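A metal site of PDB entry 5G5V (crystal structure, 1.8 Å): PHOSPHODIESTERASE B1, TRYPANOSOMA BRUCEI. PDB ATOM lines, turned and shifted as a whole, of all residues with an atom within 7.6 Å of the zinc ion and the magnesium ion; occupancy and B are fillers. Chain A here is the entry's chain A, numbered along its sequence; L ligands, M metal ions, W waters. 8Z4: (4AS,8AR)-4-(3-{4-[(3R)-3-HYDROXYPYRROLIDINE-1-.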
ATOM      1  N   TYR A 110     -19.519  11.951   6.487  1.00  0.00           N
ATOM      2  CA  TYR A 110     -20.146  13.173   5.928  1.00  0.00           C
ATOM      3  C   TYR A 110     -21.187  12.931   4.806  1.00  0.00           C
ATOM      4  O   TYR A 110     -22.315  13.457   4.886  1.00  0.00           O
ATOM      5  CB  TYR A 110     -19.062  14.130   5.437  1.00  0.00           C
ATOM      6  CG  TYR A 110     -19.598  15.442   4.871  1.00  0.00           C
ATOM      7  CD1 TYR A 110     -19.937  16.504   5.713  1.00  0.00           C
ATOM      8  CD2 TYR A 110     -19.767  15.603   3.497  1.00  0.00           C
ATOM      9  CE1 TYR A 110     -20.428  17.705   5.179  1.00  0.00           C
ATOM     10  CE2 TYR A 110     -20.274  16.785   2.961  1.00  0.00           C
ATOM     11  CZ  TYR A 110     -20.600  17.837   3.811  1.00  0.00           C
ATOM     12  OH  TYR A 110     -21.074  19.010   3.252  1.00  0.00           O
ATOM     13  N   HIS A 111     -20.827  12.150   3.791  1.00  0.00           N
ATOM     14  CA  HIS A 111     -21.661  11.997   2.572  1.00  0.00           C
ATOM     15  C   HIS A 111     -22.774  10.972   2.758  1.00  0.00           C
ATOM     16  O   HIS A 111     -22.903   9.966   2.030  1.00  0.00           O
ATOM     17  CB  HIS A 111     -20.806  11.707   1.323  1.00  0.00           C
ATOM     18  CG  HIS A 111     -20.031  12.897   0.845  1.00  0.00           C
ATOM     19  ND1 HIS A 111     -18.694  13.069   1.084  1.00  0.00           N
ATOM     20  CD2 HIS A 111     -20.428  13.987   0.126  1.00  0.00           C
ATOM     21  CE1 HIS A 111     -18.292  14.219   0.555  1.00  0.00           C
ATOM     22  NE2 HIS A 111     -19.333  14.795  -0.029  1.00  0.00           N
ATOM     23  N   HIS A 115     -26.492  14.620   5.161  1.00  0.00           N
ATOM     24  CA  HIS A 115     -26.014  15.635   4.210  1.00  0.00           C
ATOM     25  C   HIS A 115     -27.084  15.974   3.150  1.00  0.00           C
ATOM     26  O   HIS A 115     -27.284  17.144   2.830  1.00  0.00           O
ATOM     27  CB  HIS A 115     -24.702  15.184   3.542  1.00  0.00           C
ATOM     28  CG  HIS A 115     -24.318  15.959   2.317  1.00  0.00           C
ATOM     29  ND1 HIS A 115     -23.949  17.291   2.362  1.00  0.00           N
ATOM     30  CD2 HIS A 115     -24.221  15.583   1.029  1.00  0.00           C
ATOM     31  CE1 HIS A 115     -23.645  17.696   1.141  1.00  0.00           C
ATOM     32  NE2 HIS A 115     -23.802  16.674   0.318  1.00  0.00           N
ATOM     33  N   VAL A 116     -27.743  14.953   2.607  1.00  0.00           N
ATOM     34  CA  VAL A 116     -28.705  15.214   1.527  1.00  0.00           C
ATOM     35  C   VAL A 116     -30.013  15.841   2.001  1.00  0.00           C
ATOM     36  O   VAL A 116     -30.587  16.686   1.284  1.00  0.00           O
ATOM     37  CB  VAL A 116     -28.925  13.999   0.575  1.00  0.00           C
ATOM     38  CG1 VAL A 116     -27.583  13.490   0.046  1.00  0.00           C
ATOM     39  CG2 VAL A 116     -29.737  12.876   1.210  1.00  0.00           C
ATOM     40  N   VAL A 119     -29.060  19.464   2.378  1.00  0.00           N
ATOM     41  CA  VAL A 119     -29.041  20.150   1.064  1.00  0.00           C
ATOM     42  C   VAL A 119     -30.479  20.476   0.592  1.00  0.00           C
ATOM     43  O   VAL A 119     -30.740  21.574   0.089  1.00  0.00           O
ATOM     44  CB  VAL A 119     -28.218  19.345  -0.004  1.00  0.00           C
ATOM     45  CG1 VAL A 119     -28.367  19.931  -1.398  1.00  0.00           C
ATOM     46  CG2 VAL A 119     -26.745  19.334   0.372  1.00  0.00           C
ATOM     47  N   ALA A 148     -32.003  17.095  -4.879  1.00  0.00           N
ATOM     48  CA  ALA A 148     -31.214  17.172  -3.651  1.00  0.00           C
ATOM     49  C   ALA A 148     -31.150  15.826  -2.910  1.00  0.00           C
ATOM     50  O   ALA A 148     -30.100  15.473  -2.386  1.00  0.00           O
ATOM     51  CB  ALA A 148     -31.759  18.231  -2.692  1.00  0.00           C
ATOM     52  N   HIS A 151     -28.729  13.231  -4.911  1.00  0.00           N
ATOM     53  CA  HIS A 151     -27.533  13.735  -5.594  1.00  0.00           C
ATOM     54  C   HIS A 151     -26.202  13.095  -5.160  1.00  0.00           C
ATOM     55  O   HIS A 151     -25.201  13.280  -5.855  1.00  0.00           O
ATOM     56  CB  HIS A 151     -27.449  15.267  -5.486  1.00  0.00           C
ATOM     57  CG  HIS A 151     -26.761  15.767  -4.251  1.00  0.00           C
ATOM     58  ND1 HIS A 151     -27.419  15.933  -3.052  1.00  0.00           N
ATOM     59  CD2 HIS A 151     -25.475  16.096  -4.027  1.00  0.00           C
ATOM     60  CE1 HIS A 151     -26.554  16.366  -2.151  1.00  0.00           C
ATOM     61  NE2 HIS A 151     -25.371  16.463  -2.721  1.00  0.00           N
ATOM     62  N   ASP A 152     -26.181  12.389  -4.022  1.00  0.00           N
ATOM     63  CA  ASP A 152     -24.978  11.680  -3.547  1.00  0.00           C
ATOM     64  C   ASP A 152     -25.210  10.179  -3.283  1.00  0.00           C
ATOM     65  O   ASP A 152     -24.447   9.567  -2.526  1.00  0.00           O
ATOM     66  CB  ASP A 152     -24.414  12.385  -2.283  1.00  0.00           C
ATOM     67  CG  ASP A 152     -23.445  13.515  -2.591  1.00  0.00           C
ATOM     68  OD1 ASP A 152     -22.758  13.453  -3.622  1.00  0.00           O
ATOM     69  OD2 ASP A 152     -23.347  14.453  -1.764  1.00  0.00           O
ATOM     70  N   LEU A 153     -26.210   9.557  -3.926  1.00  0.00           N
ATOM     71  CA  LEU A 153     -26.590   8.154  -3.618  1.00  0.00           C
ATOM     72  C   LEU A 153     -25.382   7.171  -3.625  1.00  0.00           C
ATOM     73  O   LEU A 153     -24.612   7.166  -4.579  1.00  0.00           O
ATOM     74  CB  LEU A 153     -27.646   7.624  -4.601  1.00  0.00           C
ATOM     75  CG  LEU A 153     -29.113   8.120  -4.456  1.00  0.00           C
ATOM     76  CD1 LEU A 153     -29.936   7.848  -5.704  1.00  0.00           C
ATOM     77  CD2 LEU A 153     -29.804   7.522  -3.243  1.00  0.00           C
ATOM     78  N   HIS A 155     -22.594   7.114  -1.975  1.00  0.00           N
ATOM     79  CA  HIS A 155     -21.260   7.730  -1.827  1.00  0.00           C
ATOM     80  C   HIS A 155     -20.461   6.906  -0.779  1.00  0.00           C
ATOM     81  O   HIS A 155     -20.980   6.602   0.308  1.00  0.00           O
ATOM     82  CB  HIS A 155     -21.392   9.186  -1.358  1.00  0.00           C
ATOM     83  CG  HIS A 155     -20.250  10.080  -1.721  1.00  0.00           C
ATOM     84  ND1 HIS A 155     -18.969   9.904  -1.252  1.00  0.00           N
ATOM     85  CD2 HIS A 155     -20.207  11.230  -2.453  1.00  0.00           C
ATOM     86  CE1 HIS A 155     -18.177  10.860  -1.711  1.00  0.00           C
ATOM     87  NE2 HIS A 155     -18.915  11.678  -2.446  1.00  0.00           N
ATOM     88  N   LEU A 183     -18.208   9.357  -9.628  1.00  0.00           N
ATOM     89  CA  LEU A 183     -19.210   9.411  -8.566  1.00  0.00           C
ATOM     90  C   LEU A 183     -20.573   9.850  -9.097  1.00  0.00           C
ATOM     91  O   LEU A 183     -21.591   9.211  -8.825  1.00  0.00           O
ATOM     92  CB  LEU A 183     -18.792  10.384  -7.482  1.00  0.00           C
ATOM     93  CG  LEU A 183     -17.846   9.883  -6.380  1.00  0.00           C
ATOM     94  CD1 LEU A 183     -17.222  11.056  -5.660  1.00  0.00           C
ATOM     95  CD2 LEU A 183     -18.613   9.018  -5.410  1.00  0.00           C
ATOM     96  N   GLU A 184     -20.573  10.924  -9.876  1.00  0.00           N
ATOM     97  CA  GLU A 184     -21.829  11.584 -10.267  1.00  0.00           C
ATOM     98  C   GLU A 184     -22.642  10.748 -11.257  1.00  0.00           C
ATOM     99  O   GLU A 184     -23.880  10.678 -11.138  1.00  0.00           O
ATOM    100  CB  GLU A 184     -21.562  13.022 -10.721  1.00  0.00           C
ATOM    101  CG  GLU A 184     -21.015  13.944  -9.615  1.00  0.00           C
ATOM    102  CD  GLU A 184     -19.532  13.748  -9.235  1.00  0.00           C
ATOM    103  OE1 GLU A 184     -18.747  13.195 -10.044  1.00  0.00           O
ATOM    104  OE2 GLU A 184     -19.141  14.176  -8.120  1.00  0.00           O
ATOM    105  N   HIS A 187     -24.309   8.125  -9.038  1.00  0.00           N
ATOM    106  CA  HIS A 187     -25.472   8.668  -8.337  1.00  0.00           C
ATOM    107  C   HIS A 187     -26.712   8.699  -9.289  1.00  0.00           C
ATOM    108  O   HIS A 187     -27.825   8.291  -8.895  1.00  0.00           O
ATOM    109  CB  HIS A 187     -25.231  10.084  -7.751  1.00  0.00           C
ATOM    110  CG  HIS A 187     -23.998  10.236  -6.911  1.00  0.00           C
ATOM    111  ND1 HIS A 187     -23.581   9.298  -5.985  1.00  0.00           N
ATOM    112  CD2 HIS A 187     -23.120  11.261  -6.828  1.00  0.00           C
ATOM    113  CE1 HIS A 187     -22.475   9.732  -5.399  1.00  0.00           C
ATOM    114  NE2 HIS A 187     -22.165  10.910  -5.894  1.00  0.00           N
ATOM    115  N   VAL A 222     -27.170  16.818 -11.238  1.00  0.00           N
ATOM    116  CA  VAL A 222     -26.266  15.898 -10.500  1.00  0.00           C
ATOM    117  C   VAL A 222     -24.861  15.883 -11.142  1.00  0.00           C
ATOM    118  O   VAL A 222     -23.843  16.017 -10.463  1.00  0.00           O
ATOM    119  CB  VAL A 222     -26.846  14.468 -10.390  1.00  0.00           C
ATOM    120  CG1 VAL A 222     -25.843  13.523  -9.721  1.00  0.00           C
ATOM    121  CG2 VAL A 222     -28.169  14.489  -9.618  1.00  0.00           C
ATOM    122  N   THR A 225     -22.528  18.736 -10.135  1.00  0.00           N
ATOM    123  CA  THR A 225     -21.950  18.822  -8.780  1.00  0.00           C
ATOM    124  C   THR A 225     -20.492  18.305  -8.678  1.00  0.00           C
ATOM    125  O   THR A 225     -19.882  18.423  -7.603  1.00  0.00           O
ATOM    126  CB  THR A 225     -22.813  18.088  -7.727  1.00  0.00           C
ATOM    127  OG1 THR A 225     -22.961  16.708  -8.083  1.00  0.00           O
ATOM    128  CG2 THR A 225     -24.181  18.767  -7.585  1.00  0.00           C
ATOM    129  N   ASP A 226     -19.936  17.765  -9.756  1.00  0.00           N
ATOM    130  CA  ASP A 226     -18.502  17.379  -9.785  1.00  0.00           C
ATOM    131  C   ASP A 226     -17.680  18.668  -9.698  1.00  0.00           C
ATOM    132  O   ASP A 226     -17.771  19.501 -10.599  1.00  0.00           O
ATOM    133  CB  ASP A 226     -18.210  16.592 -11.066  1.00  0.00           C
ATOM    134  CG  ASP A 226     -16.755  16.200 -11.212  1.00  0.00           C
ATOM    135  OD1 ASP A 226     -15.910  16.605 -10.407  1.00  0.00           O
ATOM    136  OD2 ASP A 226     -16.468  15.466 -12.183  1.00  0.00           O
ATOM    137  N   MET A 227     -16.919  18.849  -8.628  1.00  0.00           N
ATOM    138  CA  MET A 227     -16.139  20.103  -8.432  1.00  0.00           C
ATOM    139  C   MET A 227     -15.036  20.370  -9.476  1.00  0.00           C
ATOM    140  O   MET A 227     -14.596  21.519  -9.638  1.00  0.00           O
ATOM    141  CB  MET A 227     -15.610  20.231  -6.998  1.00  0.00           C
ATOM    142  CG  MET A 227     -16.712  20.469  -5.947  1.00  0.00           C
ATOM    143  SD  MET A 227     -17.590  22.036  -6.109  1.00  0.00           S
ATOM    144  CE  MET A 227     -16.401  23.205  -5.444  1.00  0.00           C
ATOM    145  N   LEU A 260     -28.342  23.880  -6.965  1.00  0.00           N
ATOM    146  CA  LEU A 260     -27.912  22.603  -6.383  1.00  0.00           C
ATOM    147  C   LEU A 260     -26.459  22.702  -5.885  1.00  0.00           C
ATOM    148  O   LEU A 260     -26.158  22.291  -4.755  1.00  0.00           O
ATOM    149  CB  LEU A 260     -28.070  21.422  -7.333  1.00  0.00           C
ATOM    150  CG  LEU A 260     -27.631  20.050  -6.762  1.00  0.00           C
ATOM    151  CD1 LEU A 260     -28.377  19.708  -5.480  1.00  0.00           C
ATOM    152  CD2 LEU A 260     -27.822  18.932  -7.773  1.00  0.00           C
ATOM    153  N   GLY A 263     -26.454  24.745  -2.600  1.00  0.00           N
ATOM    154  CA  GLY A 263     -26.830  23.885  -1.484  1.00  0.00           C
ATOM    155  C   GLY A 263     -25.689  22.962  -1.038  1.00  0.00           C
ATOM    156  O   GLY A 263     -25.452  22.758   0.163  1.00  0.00           O
ATOM    157  N   ASP A 264     -25.018  22.396  -2.027  1.00  0.00           N
ATOM    158  CA  ASP A 264     -23.952  21.419  -1.782  1.00  0.00           C
ATOM    159  C   ASP A 264     -22.761  22.003  -1.015  1.00  0.00           C
ATOM    160  O   ASP A 264     -22.147  21.282  -0.224  1.00  0.00           O
ATOM    161  CB  ASP A 264     -23.461  20.838  -3.100  1.00  0.00           C
ATOM    162  CG  ASP A 264     -22.896  19.427  -2.955  1.00  0.00           C
ATOM    163  OD1 ASP A 264     -23.264  18.683  -2.024  1.00  0.00           O
ATOM    164  OD2 ASP A 264     -22.089  19.073  -3.836  1.00  0.00           O
ATOM    165  N   ILE A 265     -22.437  23.286  -1.238  1.00  0.00           N
ATOM    166  CA  ILE A 265     -21.353  23.962  -0.485  1.00  0.00           C
ATOM    167  C   ILE A 265     -21.838  24.990   0.563  1.00  0.00           C
ATOM    168  O   ILE A 265     -21.081  25.889   0.967  1.00  0.00           O
ATOM    169  CB  ILE A 265     -20.298  24.592  -1.436  1.00  0.00           C
ATOM    170  CG1 ILE A 265     -20.861  25.661  -2.357  1.00  0.00           C
ATOM    171  CG2 ILE A 265     -19.612  23.503  -2.262  1.00  0.00           C
ATOM    172  CD1 ILE A 265     -19.784  26.488  -3.031  1.00  0.00           C
HETATM  173  O3  8Z4 L   1     -15.045  18.289  -4.208  1.00  0.00           O
HETATM  174  C28 8Z4 L   1     -15.197  18.733  -3.072  1.00  0.00           C
HETATM  175  N   8Z4 L   1     -14.370  19.728  -2.559  1.00  0.00           N
HETATM  176  C1  8Z4 L   1     -13.282  20.344  -3.358  1.00  0.00           C
HETATM  177  C2  8Z4 L   1     -11.927  19.878  -2.863  1.00  0.00           C
HETATM  178  C   8Z4 L   1     -13.399  21.850  -3.339  1.00  0.00           C
HETATM  179  C27 8Z4 L   1     -16.269  18.181  -2.148  1.00  0.00           C
HETATM  180  C26 8Z4 L   1     -17.408  17.423  -2.833  1.00  0.00           C
HETATM  181  C25 8Z4 L   1     -18.485  18.314  -3.355  1.00  0.00           C
HETATM  182  C24 8Z4 L   1     -18.588  19.583  -3.032  1.00  0.00           C
HETATM  183  C23 8Z4 L   1     -17.683  20.270  -2.067  1.00  0.00           C
HETATM  184  C22 8Z4 L   1     -16.794  19.311  -1.230  1.00  0.00           C
HETATM  185  C3  8Z4 L   1     -15.581  20.020  -0.644  1.00  0.00           C
HETATM  186  N1  8Z4 L   1     -14.483  20.206  -1.281  1.00  0.00           N
HETATM  187  C4  8Z4 L   1     -15.643  20.574   0.733  1.00  0.00           C
HETATM  188  C21 8Z4 L   1     -14.461  20.702   1.478  1.00  0.00           C
HETATM  189  C9  8Z4 L   1     -14.509  21.272   2.738  1.00  0.00           C
HETATM  190  C7  8Z4 L   1     -15.748  21.660   3.287  1.00  0.00           C
HETATM  191  O   8Z4 L   1     -15.695  22.169   4.559  1.00  0.00           O
HETATM  192  C8  8Z4 L   1     -16.841  22.823   5.106  1.00  0.00           C
HETATM  193  C6  8Z4 L   1     -16.922  21.520   2.541  1.00  0.00           C
HETATM  194  C5  8Z4 L   1     -16.860  20.988   1.270  1.00  0.00           C
HETATM  195  C10 8Z4 L   1     -13.359  21.326   3.551  1.00  0.00           C
HETATM  196  C20 8Z4 L   1     -12.680  22.516   3.830  1.00  0.00           C
HETATM  197  C19 8Z4 L   1     -11.627  22.535   4.720  1.00  0.00           C
HETATM  198  C13 8Z4 L   1     -11.222  21.370   5.382  1.00  0.00           C
HETATM  199  C12 8Z4 L   1     -11.936  20.193   5.147  1.00  0.00           C
HETATM  200  C11 8Z4 L   1     -12.983  20.180   4.243  1.00  0.00           C
HETATM  201  C14 8Z4 L   1     -10.145  21.414   6.411  1.00  0.00           C
HETATM  202  O2  8Z4 L   1     -10.154  22.326   7.253  1.00  0.00           O
HETATM  203  N2  8Z4 L   1      -9.267  20.401   6.520  1.00  0.00           N
HETATM  204  C18 8Z4 L   1      -8.172  20.445   7.509  1.00  0.00           C
HETATM  205  C17 8Z4 L   1      -7.103  19.639   6.778  1.00  0.00           C
HETATM  206  O1  8Z4 L   1      -6.569  20.396   5.702  1.00  0.00           O
HETATM  207  C16 8Z4 L   1      -7.937  18.482   6.272  1.00  0.00           C
HETATM  208  C15 8Z4 L   1      -9.205  19.141   5.766  1.00  0.00           C
HETATM  209 ZN    ZN M   1     -23.210  16.566  -1.899  1.00  0.00          ZN
HETATM  210 MG    MG M   2     -21.431  14.815  -4.656  1.00  0.00          MG
HETATM  211  O   HOH W   1     -22.855  14.581  -6.310  1.00  0.00           O
HETATM  212  O   HOH W   2     -22.339  16.510  -3.802  1.00  0.00           O
HETATM  213  O   HOH W   3     -21.129  16.799  -1.241  1.00  0.00           O
HETATM  214  O   HOH W   4     -19.845  14.898  -3.098  1.00  0.00           O
HETATM  215  O   HOH W   5     -20.150  16.044  -6.119  1.00  0.00           O
HETATM  216  O   HOH W   6     -20.404  13.032  -5.522  1.00  0.00           O
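A ring nitrogen (ND1) of His 151 sits at hydrogen-bond distance from the backbone carbonyl oxygen (O) of Ala 148, 2.8 Å away. ND1 of His 115 lies within hydrogen-bond range of OH of Tyr 110. A ring nitrogen (NE2) of His 187 sits close to the side-chain carboxylate of Asp 152.
One residue has an atom within 4 Å of the magnesium ion: Asp 152. The nearest printed residue that does not touch the magnesium ion is His 187 (4.2 Å).
Water W5 bridges the backbone carbonyl oxygen of Thr 225 (2.8 Å) and the side-chain carboxylate of Glu 184 (2.9 Å). Water W6 lies within hydrogen-bond range of NE2 of His 187 (2.8 Å) and OE2 of Glu 184 (3.1 Å). Water W1 lies within hydrogen-bond range of the backbone carbonyl oxygen (O) of His 151 (2.7 Å) and the side-chain hydroxyl (OG1) of Thr 225 (2.8 Å). Water W4 bridges a ring nitrogen (NE2) of His 111 (3.1 Å) and a ring nitrogen (NE2) of His 155 (3.4 Å).
Of the 21 residues printed, 4 come within 4 Å of the zinc ion. The nearest printed residue that does not touch the zinc ion is His 111 (4.3 Å).
The zinc ion is bound by water W2 (2.1 Å), the side-chain carboxylate (OD1) of Asp 264 (2.1 Å), the side-chain carboxylate (OD2) of Asp 152 (2.1 Å), water W3 (2.2 Å), a ring nitrogen (NE2) of His 115 (2.3 Å) and a ring nitrogen (NE2) of His 151 (2.3 Å). The zinc ion has six donor atoms within binding distance.
The magnesium ion is bound by water W2 (2.1 Å), the side-chain carboxylate (OD1) of Asp 152 (2.2 Å), water W1 (2.2 Å), water W4 (2.2 Å), water W6 (2.2 Å) and water W5 (2.3 Å).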
